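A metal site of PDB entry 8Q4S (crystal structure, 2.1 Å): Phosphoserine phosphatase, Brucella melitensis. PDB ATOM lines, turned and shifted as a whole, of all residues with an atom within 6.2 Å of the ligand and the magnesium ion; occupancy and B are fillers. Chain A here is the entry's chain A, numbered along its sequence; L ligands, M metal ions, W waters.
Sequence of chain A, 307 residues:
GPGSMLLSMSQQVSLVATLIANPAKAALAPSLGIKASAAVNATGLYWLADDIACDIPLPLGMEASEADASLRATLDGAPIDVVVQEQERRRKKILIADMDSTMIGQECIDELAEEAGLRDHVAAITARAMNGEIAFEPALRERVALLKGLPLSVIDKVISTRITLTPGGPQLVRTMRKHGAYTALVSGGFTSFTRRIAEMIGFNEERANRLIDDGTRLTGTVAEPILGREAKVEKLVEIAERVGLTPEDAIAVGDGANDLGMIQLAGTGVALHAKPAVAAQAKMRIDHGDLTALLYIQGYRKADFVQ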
ATOM      1  N   ASP A  98      14.739 -14.502   3.550  1.00  0.00           N
ATOM      2  CA  ASP A  98      15.865 -15.235   4.081  1.00  0.00           C
ATOM      3  C   ASP A  98      15.969 -15.034   5.598  1.00  0.00           C
ATOM      4  O   ASP A  98      15.479 -14.039   6.135  1.00  0.00           O
ATOM      5  CB  ASP A  98      17.140 -14.734   3.405  1.00  0.00           C
ATOM      6  CG  ASP A  98      18.352 -15.461   3.873  1.00  0.00           C
ATOM      7  OD1 ASP A  98      18.230 -16.694   3.996  1.00  0.00           O
ATOM      8  OD2 ASP A  98      19.392 -14.822   4.130  1.00  0.00           O
ATOM      9  N   MET A  99      16.604 -15.984   6.301  1.00  0.00           N
ATOM     10  CA  MET A  99      16.845 -15.806   7.744  1.00  0.00           C
ATOM     11  C   MET A  99      18.219 -15.210   8.044  1.00  0.00           C
ATOM     12  O   MET A  99      18.304 -14.084   8.544  1.00  0.00           O
ATOM     13  CB  MET A  99      16.691 -17.127   8.504  1.00  0.00           C
ATOM     14  CG  MET A  99      16.756 -16.917  10.034  1.00  0.00           C
ATOM     15  SD  MET A  99      16.648 -18.397  11.077  1.00  0.00           S
ATOM     16  CE  MET A  99      18.063 -19.349  10.474  1.00  0.00           C
ATOM     17  N   ASP A 100      19.286 -15.967   7.805  1.00  0.00           N
ATOM     18  CA  ASP A 100      20.611 -15.609   8.290  1.00  0.00           C
ATOM     19  C   ASP A 100      21.048 -14.266   7.714  1.00  0.00           C
ATOM     20  O   ASP A 100      21.000 -14.055   6.498  1.00  0.00           O
ATOM     21  CB  ASP A 100      21.627 -16.689   7.907  1.00  0.00           C
ATOM     22  CG  ASP A 100      21.568 -17.918   8.835  1.00  0.00           C
ATOM     23  OD1 ASP A 100      21.123 -17.819   9.981  1.00  0.00           O
ATOM     24  OD2 ASP A 100      21.971 -18.997   8.401  1.00  0.00           O
ATOM     25  N   SER A 101      21.463 -13.367   8.598  1.00  0.00           N
ATOM     26  CA  SER A 101      21.953 -12.026   8.267  1.00  0.00           C
ATOM     27  C   SER A 101      20.886 -11.152   7.669  1.00  0.00           C
ATOM     28  O   SER A 101      21.184 -10.068   7.175  1.00  0.00           O
ATOM     29  CB  SER A 101      23.144 -12.060   7.290  1.00  0.00           C
ATOM     30  OG  SER A 101      24.278 -12.584   7.950  1.00  0.00           O
ATOM     31  N   THR A 102      19.628 -11.607   7.666  1.00  0.00           N
ATOM     32  CA  THR A 102      18.528 -10.818   7.124  1.00  0.00           C
ATOM     33  C   THR A 102      17.517 -10.572   8.232  1.00  0.00           C
ATOM     34  O   THR A 102      17.429  -9.430   8.705  1.00  0.00           O
ATOM     35  CB  THR A 102      17.929 -11.525   5.904  1.00  0.00           C
ATOM     36  OG1 THR A 102      18.933 -11.653   4.890  1.00  0.00           O
ATOM     37  CG2 THR A 102      16.757 -10.767   5.317  1.00  0.00           C
ATOM     38  N   GLU A 107      24.893 -15.688  11.424  1.00  0.00           N
ATOM     39  CA  GLU A 107      24.857 -16.880  10.578  1.00  0.00           C
ATOM     40  C   GLU A 107      24.788 -18.061  11.534  1.00  0.00           C
ATOM     41  O   GLU A 107      25.747 -18.316  12.271  1.00  0.00           O
ATOM     42  CB  GLU A 107      26.100 -16.963   9.701  1.00  0.00           C
ATOM     43  CG  GLU A 107      26.258 -15.835   8.673  1.00  0.00           C
ATOM     44  CD  GLU A 107      25.353 -16.043   7.473  1.00  0.00           C
ATOM     45  OE1 GLU A 107      24.952 -17.200   7.236  1.00  0.00           O
ATOM     46  OE2 GLU A 107      25.032 -15.061   6.788  1.00  0.00           O
ATOM     47  N   CYS A 108      23.650 -18.776  11.515  1.00  0.00           N
ATOM     48  CA  CYS A 108      23.450 -19.895  12.428  1.00  0.00           C
ATOM     49  C   CYS A 108      24.573 -20.919  12.316  1.00  0.00           C
ATOM     50  O   CYS A 108      25.002 -21.502  13.328  1.00  0.00           O
ATOM     51  CB  CYS A 108      22.070 -20.542  12.177  1.00  0.00           C
ATOM     52  SG  CYS A 108      21.669 -21.254  10.486  1.00  0.00           S
ATOM     53  N   ILE A 109      25.106 -21.119  11.105  1.00  0.00           N
ATOM     54  CA  ILE A 109      26.145 -22.111  10.895  1.00  0.00           C
ATOM     55  C   ILE A 109      27.476 -21.631  11.471  1.00  0.00           C
ATOM     56  O   ILE A 109      28.262 -22.438  11.977  1.00  0.00           O
ATOM     57  CB  ILE A 109      26.271 -22.467   9.401  1.00  0.00           C
ATOM     58  CG1 ILE A 109      27.157 -23.694   9.241  1.00  0.00           C
ATOM     59  CG2 ILE A 109      26.827 -21.319   8.582  1.00  0.00           C
ATOM     60  CD1 ILE A 109      26.582 -24.671   8.275  1.00  0.00           C
ATOM     61  N   THR A 126      31.488 -19.449   4.679  1.00  0.00           N
ATOM     62  CA  THR A 126      30.187 -18.802   4.586  1.00  0.00           C
ATOM     63  C   THR A 126      30.272 -17.525   3.774  1.00  0.00           C
ATOM     64  O   THR A 126      29.440 -17.275   2.886  1.00  0.00           O
ATOM     65  CB  THR A 126      29.654 -18.505   5.990  1.00  0.00           C
ATOM     66  OG1 THR A 126      29.600 -19.729   6.724  1.00  0.00           O
ATOM     67  CG2 THR A 126      28.277 -17.897   5.913  1.00  0.00           C
ATOM     68  N   ALA A 129      30.461 -18.389   0.170  1.00  0.00           N
ATOM     69  CA  ALA A 129      29.186 -18.917  -0.327  1.00  0.00           C
ATOM     70  C   ALA A 129      28.171 -17.802  -0.505  1.00  0.00           C
ATOM     71  O   ALA A 129      27.461 -17.746  -1.518  1.00  0.00           O
ATOM     72  CB  ALA A 129      28.630 -19.979   0.617  1.00  0.00           C
ATOM     73  N   MET A 130      28.088 -16.891   0.476  1.00  0.00           N
ATOM     74  CA  MET A 130      27.104 -15.828   0.349  1.00  0.00           C
ATOM     75  C   MET A 130      27.492 -14.810  -0.707  1.00  0.00           C
ATOM     76  O   MET A 130      26.618 -14.164  -1.275  1.00  0.00           O
ATOM     77  CB  MET A 130      26.878 -15.180   1.724  1.00  0.00           C
ATOM     78  CG  MET A 130      26.197 -16.166   2.734  1.00  0.00           C
ATOM     79  SD  MET A 130      24.566 -16.810   2.170  1.00  0.00           S
ATOM     80  CE  MET A 130      25.020 -18.350   1.349  1.00  0.00           C
ATOM     81  N   PHE A 136      26.072 -23.178  -3.175  1.00  0.00           N
ATOM     82  CA  PHE A 136      25.584 -23.291  -1.805  1.00  0.00           C
ATOM     83  C   PHE A 136      25.733 -24.712  -1.260  1.00  0.00           C
ATOM     84  O   PHE A 136      26.219 -24.911  -0.139  1.00  0.00           O
ATOM     85  CB  PHE A 136      24.129 -22.854  -1.711  1.00  0.00           C
ATOM     86  CG  PHE A 136      23.611 -22.907  -0.315  1.00  0.00           C
ATOM     87  CD1 PHE A 136      23.954 -21.909   0.587  1.00  0.00           C
ATOM     88  CD2 PHE A 136      22.836 -23.974   0.110  1.00  0.00           C
ATOM     89  CE1 PHE A 136      23.502 -21.951   1.895  1.00  0.00           C
ATOM     90  CE2 PHE A 136      22.370 -24.020   1.420  1.00  0.00           C
ATOM     91  CZ  PHE A 136      22.712 -22.997   2.320  1.00  0.00           C
ATOM     92  N   LEU A 140      27.632 -25.823   2.109  1.00  0.00           N
ATOM     93  CA  LEU A 140      26.905 -26.279   3.288  1.00  0.00           C
ATOM     94  C   LEU A 140      27.454 -27.614   3.783  1.00  0.00           C
ATOM     95  O   LEU A 140      27.697 -27.786   4.983  1.00  0.00           O
ATOM     96  CB  LEU A 140      25.421 -26.393   2.976  1.00  0.00           C
ATOM     97  CG  LEU A 140      24.499 -26.707   4.142  1.00  0.00           C
ATOM     98  CD1 LEU A 140      24.570 -25.595   5.202  1.00  0.00           C
ATOM     99  CD2 LEU A 140      23.072 -26.876   3.603  1.00  0.00           C
ATOM    100  N   ARG A 143      30.796 -27.240   5.570  1.00  0.00           N
ATOM    101  CA  ARG A 143      30.726 -26.618   6.887  1.00  0.00           C
ATOM    102  C   ARG A 143      30.019 -27.518   7.899  1.00  0.00           C
ATOM    103  O   ARG A 143      30.462 -27.646   9.031  1.00  0.00           O
ATOM    104  CB  ARG A 143      30.012 -25.274   6.793  1.00  0.00           C
ATOM    105  CG  ARG A 143      30.792 -24.241   5.989  1.00  0.00           C
ATOM    106  CD  ARG A 143      29.944 -23.012   5.719  1.00  0.00           C
ATOM    107  NE  ARG A 143      28.916 -23.236   4.707  1.00  0.00           N
ATOM    108  CZ  ARG A 143      27.911 -22.403   4.480  1.00  0.00           C
ATOM    109  NH1 ARG A 143      27.760 -21.299   5.194  1.00  0.00           N
ATOM    110  NH2 ARG A 143      27.026 -22.675   3.524  1.00  0.00           N
ATOM    111  N   VAL A 186      12.184 -18.480   4.581  1.00  0.00           N
ATOM    112  CA  VAL A 186      12.705 -19.536   3.736  1.00  0.00           C
ATOM    113  C   VAL A 186      14.221 -19.407   3.700  1.00  0.00           C
ATOM    114  O   VAL A 186      14.753 -18.415   3.193  1.00  0.00           O
ATOM    115  CB  VAL A 186      12.083 -19.478   2.324  1.00  0.00           C
ATOM    116  CG1 VAL A 186      12.625 -20.576   1.438  1.00  0.00           C
ATOM    117  CG2 VAL A 186      10.552 -19.575   2.427  1.00  0.00           C
ATOM    118  N   SER A 187      14.909 -20.428   4.217  1.00  0.00           N
ATOM    119  CA  SER A 187      16.292 -20.309   4.653  1.00  0.00           C
ATOM    120  C   SER A 187      17.130 -21.503   4.192  1.00  0.00           C
ATOM    121  O   SER A 187      16.635 -22.640   4.169  1.00  0.00           O
ATOM    122  CB  SER A 187      16.332 -20.180   6.196  1.00  0.00           C
ATOM    123  OG  SER A 187      17.638 -20.326   6.729  1.00  0.00           O
ATOM    124  N   GLY A 188      18.385 -21.244   3.832  1.00  0.00           N
ATOM    125  CA  GLY A 188      19.328 -22.325   3.650  1.00  0.00           C
ATOM    126  C   GLY A 188      19.863 -22.867   4.951  1.00  0.00           C
ATOM    127  O   GLY A 188      20.681 -23.794   4.936  1.00  0.00           O
ATOM    128  N   GLY A 189      19.433 -22.304   6.091  1.00  0.00           N
ATOM    129  CA  GLY A 189      19.865 -22.749   7.395  1.00  0.00           C
ATOM    130  C   GLY A 189      19.041 -23.925   7.873  1.00  0.00           C
ATOM    131  O   GLY A 189      18.575 -24.736   7.072  1.00  0.00           O
ATOM    132  N   PHE A 190      18.817 -24.000   9.189  1.00  0.00           N
ATOM    133  CA  PHE A 190      18.327 -25.224   9.805  1.00  0.00           C
ATOM    134  C   PHE A 190      16.976 -25.031  10.485  1.00  0.00           C
ATOM    135  O   PHE A 190      16.716 -24.018  11.143  1.00  0.00           O
ATOM    136  CB  PHE A 190      19.367 -25.744  10.782  1.00  0.00           C
ATOM    137  CG  PHE A 190      20.752 -25.793  10.172  1.00  0.00           C
ATOM    138  CD1 PHE A 190      20.999 -26.578   9.051  1.00  0.00           C
ATOM    139  CD2 PHE A 190      21.778 -25.009  10.673  1.00  0.00           C
ATOM    140  CE1 PHE A 190      22.258 -26.623   8.452  1.00  0.00           C
ATOM    141  CE2 PHE A 190      23.041 -25.036  10.090  1.00  0.00           C
ATOM    142  CZ  PHE A 190      23.280 -25.841   8.974  1.00  0.00           C
ATOM    143  N   THR A 194      14.986 -22.027  12.384  1.00  0.00           N
ATOM    144  CA  THR A 194      13.903 -21.266  11.743  1.00  0.00           C
ATOM    145  C   THR A 194      12.568 -21.455  12.459  1.00  0.00           C
ATOM    146  O   THR A 194      11.761 -20.525  12.494  1.00  0.00           O
ATOM    147  CB  THR A 194      13.721 -21.676  10.277  1.00  0.00           C
ATOM    148  OG1 THR A 194      13.521 -23.099  10.196  1.00  0.00           O
ATOM    149  CG2 THR A 194      14.920 -21.254   9.432  1.00  0.00           C
ATOM    150  N   LYS A 232      14.684 -21.954  -3.218  1.00  0.00           N
ATOM    151  CA  LYS A 232      13.951 -20.765  -2.817  1.00  0.00           C
ATOM    152  C   LYS A 232      13.012 -20.296  -3.921  1.00  0.00           C
ATOM    153  O   LYS A 232      11.881 -19.882  -3.658  1.00  0.00           O
ATOM    154  CB  LYS A 232      14.928 -19.643  -2.401  1.00  0.00           C
ATOM    155  CG  LYS A 232      15.832 -20.024  -1.205  1.00  0.00           C
ATOM    156  CD  LYS A 232      16.340 -18.789  -0.409  1.00  0.00           C
ATOM    157  CE  LYS A 232      17.432 -19.169   0.600  1.00  0.00           C
ATOM    158  NZ  LYS A 232      17.447 -18.271   1.800  1.00  0.00           N
ATOM    159  N   GLY A 254      16.687 -10.754   0.731  1.00  0.00           N
ATOM    160  CA  GLY A 254      17.802 -11.477   1.312  1.00  0.00           C
ATOM    161  C   GLY A 254      19.088 -10.696   1.110  1.00  0.00           C
ATOM    162  O   GLY A 254      19.102  -9.589   0.575  1.00  0.00           O
ATOM    163  N   ASP A 255      20.171 -11.298   1.575  1.00  0.00           N
ATOM    164  CA  ASP A 255      21.502 -10.722   1.512  1.00  0.00           C
ATOM    165  C   ASP A 255      22.479 -11.526   0.688  1.00  0.00           C
ATOM    166  O   ASP A 255      23.542 -10.998   0.332  1.00  0.00           O
ATOM    167  CB  ASP A 255      22.083 -10.591   2.931  1.00  0.00           C
ATOM    168  CG  ASP A 255      22.399 -11.960   3.548  1.00  0.00           C
ATOM    169  OD1 ASP A 255      21.495 -12.808   3.622  1.00  0.00           O
ATOM    170  OD2 ASP A 255      23.558 -12.192   3.928  1.00  0.00           O
ATOM    171  N   GLY A 256      22.172 -12.786   0.373  1.00  0.00           N
ATOM    172  CA  GLY A 256      23.174 -13.708  -0.128  1.00  0.00           C
ATOM    173  C   GLY A 256      22.904 -14.152  -1.562  1.00  0.00           C
ATOM    174  O   GLY A 256      21.825 -13.961  -2.127  1.00  0.00           O
ATOM    175  N   ASN A 258      22.495 -17.096  -2.659  1.00  0.00           N
ATOM    176  CA  ASN A 258      21.432 -18.083  -2.730  1.00  0.00           C
ATOM    177  C   ASN A 258      20.026 -17.466  -2.689  1.00  0.00           C
ATOM    178  O   ASN A 258      19.046 -18.211  -2.811  1.00  0.00           O
ATOM    179  CB  ASN A 258      21.580 -19.114  -1.618  1.00  0.00           C
ATOM    180  CG  ASN A 258      21.571 -18.492  -0.241  1.00  0.00           C
ATOM    181  OD1 ASN A 258      22.080 -17.382  -0.035  1.00  0.00           O
ATOM    182  ND2 ASN A 258      20.985 -19.198   0.727  1.00  0.00           N
ATOM    183  N   ASP A 259      19.891 -16.144  -2.557  1.00  0.00           N
ATOM    184  CA  ASP A 259      18.590 -15.477  -2.558  1.00  0.00           C
ATOM    185  C   ASP A 259      18.279 -14.829  -3.892  1.00  0.00           C
ATOM    186  O   ASP A 259      17.156 -14.345  -4.072  1.00  0.00           O
ATOM    187  CB  ASP A 259      18.513 -14.386  -1.478  1.00  0.00           C
ATOM    188  CG  ASP A 259      18.770 -14.926  -0.096  1.00  0.00           C
ATOM    189  OD1 ASP A 259      18.172 -15.976   0.215  1.00  0.00           O
ATOM    190  OD2 ASP A 259      19.557 -14.328   0.675  1.00  0.00           O
ATOM    191  N   LYS A 275      25.909  -8.786   0.230  1.00  0.00           N
ATOM    192  CA  LYS A 275      27.289  -9.008  -0.174  1.00  0.00           C
ATOM    193  C   LYS A 275      27.576  -8.211  -1.449  1.00  0.00           C
ATOM    194  O   LYS A 275      26.656  -7.913  -2.235  1.00  0.00           O
ATOM    195  CB  LYS A 275      27.535 -10.511  -0.328  1.00  0.00           C
ATOM    196  CG  LYS A 275      27.902 -11.226   0.993  1.00  0.00           C
ATOM    197  CD  LYS A 275      26.760 -11.157   2.012  1.00  0.00           C
ATOM    198  CE  LYS A 275      27.129 -11.761   3.368  1.00  0.00           C
ATOM    199  NZ  LYS A 275      26.140 -11.358   4.445  1.00  0.00           N
HETATM  200  O1  LIG L   1      20.955 -17.171   4.846  1.00  0.00           O
HETATM  201  O2  LIG L   1      18.979 -18.229   5.941  1.00  0.00           O
HETATM  202  C1  LIG L   1      21.230 -19.789   5.743  1.00  0.00           C
HETATM  203  C2  LIG L   1      24.860 -20.278   4.820  1.00  0.00           C
HETATM  204  C3  LIG L   1      23.700 -19.478   5.419  1.00  0.00           C
HETATM  205  C4  LIG L   1      22.424 -20.064   4.850  1.00  0.00           C
HETATM  206  O3  LIG L   1      25.787 -19.715   4.185  1.00  0.00           O
HETATM  207  O4  LIG L   1      24.891 -21.521   4.944  1.00  0.00           O
HETATM  208  N1  LIG L   1      23.791 -18.059   5.073  1.00  0.00           N
HETATM  209  P1  LIG L   1      20.161 -18.465   4.998  1.00  0.00           P
HETATM  210  O5  LIG L   1      19.765 -18.923   3.602  1.00  0.00           O
HETATM  211 MG    MG M   1      21.291 -14.895   4.344  1.00  0.00          MG
HETATM  212  O   HOH W   1      21.254 -15.702   2.056  1.00  0.00           O
HETATM  213  O   HOH W   2      23.418 -22.496   6.760  1.00  0.00           O
HETATM  214  O   HOH W   3      23.578 -14.929   4.625  1.00  0.00           O
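CG2 of Thr 126 touches O3 of the ligand (3.5 Å).
CE1 of Phe 136 touches O4 of the ligand, 3.4 Å away.
N of Gly 189 touches C1 of the ligand, at 3.1 Å.
Of the 27 residues printed, 13 come within 4 Å of the ligand.
OD2 of Asp 100 sits at hydrogen-bond distance from SG of Cys 108.
N of Gly 189 sits at hydrogen-bond distance from OG of Ser 187 (2.7 Å).
NH1 of Arg 143 is in hydrogen-bond range of OG1 of Thr 126 (2.9 Å).
NZ of Lys 232 lies within salt-bridge range of OD1 of Asp 259 (2.9 Å).
SD of Met 130 sits close to OD1 of Asn 258 (3.4 Å).
The backbone NH (N) of Asp 255 lies within hydrogen-bond range of the side-chain carboxylate (OD2) of Asp 259 (3.2 Å).
OD1 of Asp 255 lies close to OG1 of Thr 102.
The backbone carbonyl oxygen (O) of Val 186 sits at hydrogen-bond distance from the side-chain amino group (NZ) of Lys 232 (3.0 Å).
OD2 of Asp 98 binds the magnesium ion (1.9 Å).
The side-chain carboxylate (OD1) of Asp 255 binds the magnesium ion, 2.2 Å away.
Water W3 is bound to the magnesium ion.
The magnesium ion is bound by O of Asp 100, at 2.3 Å.
O1 of the ligand binds the magnesium ion (2.4 Å).
The magnesium ion is bound by water W1.
The side-chain hydroxyl (OG) of Ser 187 lies within hydrogen-bond range of an oxygen (O2) of the ligand (2.6 Å).
A nitrogen (N1) of the ligand is in salt-bridge range of the side-chain carboxylate (OD2) of Asp 100 (3.9 Å).
The side-chain carboxylate (OE1) of Glu 107 lies within salt-bridge range of a nitrogen (N1) of the ligand (2.6 Å).
NZ of Lys 232 is in salt-bridge range of O5 of the ligand (3.0 Å).
N of Met 99 sits at hydrogen-bond distance from O2 of the ligand (3.3 Å).
A nitrogen (N1) of the ligand sits at hydrogen-bond distance from the side-chain sulfur (SD) of Met 130 (3.3 Å).
N of Asp 100 is in hydrogen-bond range of O2 of the ligand (2.9 Å).
An oxygen (O3) of the ligand lies within salt-bridge range of the guanidinium group of Arg 143, at 2.7 Å.
The backbone NH (N) of Gly 188 sits at hydrogen-bond distance from an oxygen (O5) of the ligand (2.7 Å).
The side-chain amide nitrogen (ND2) of Asn 258 is in hydrogen-bond range of an oxygen (O5) of the ligand (3.1 Å).
The nearest printed residue that does not touch the magnesium ion is Thr 102 (4.05 Å).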
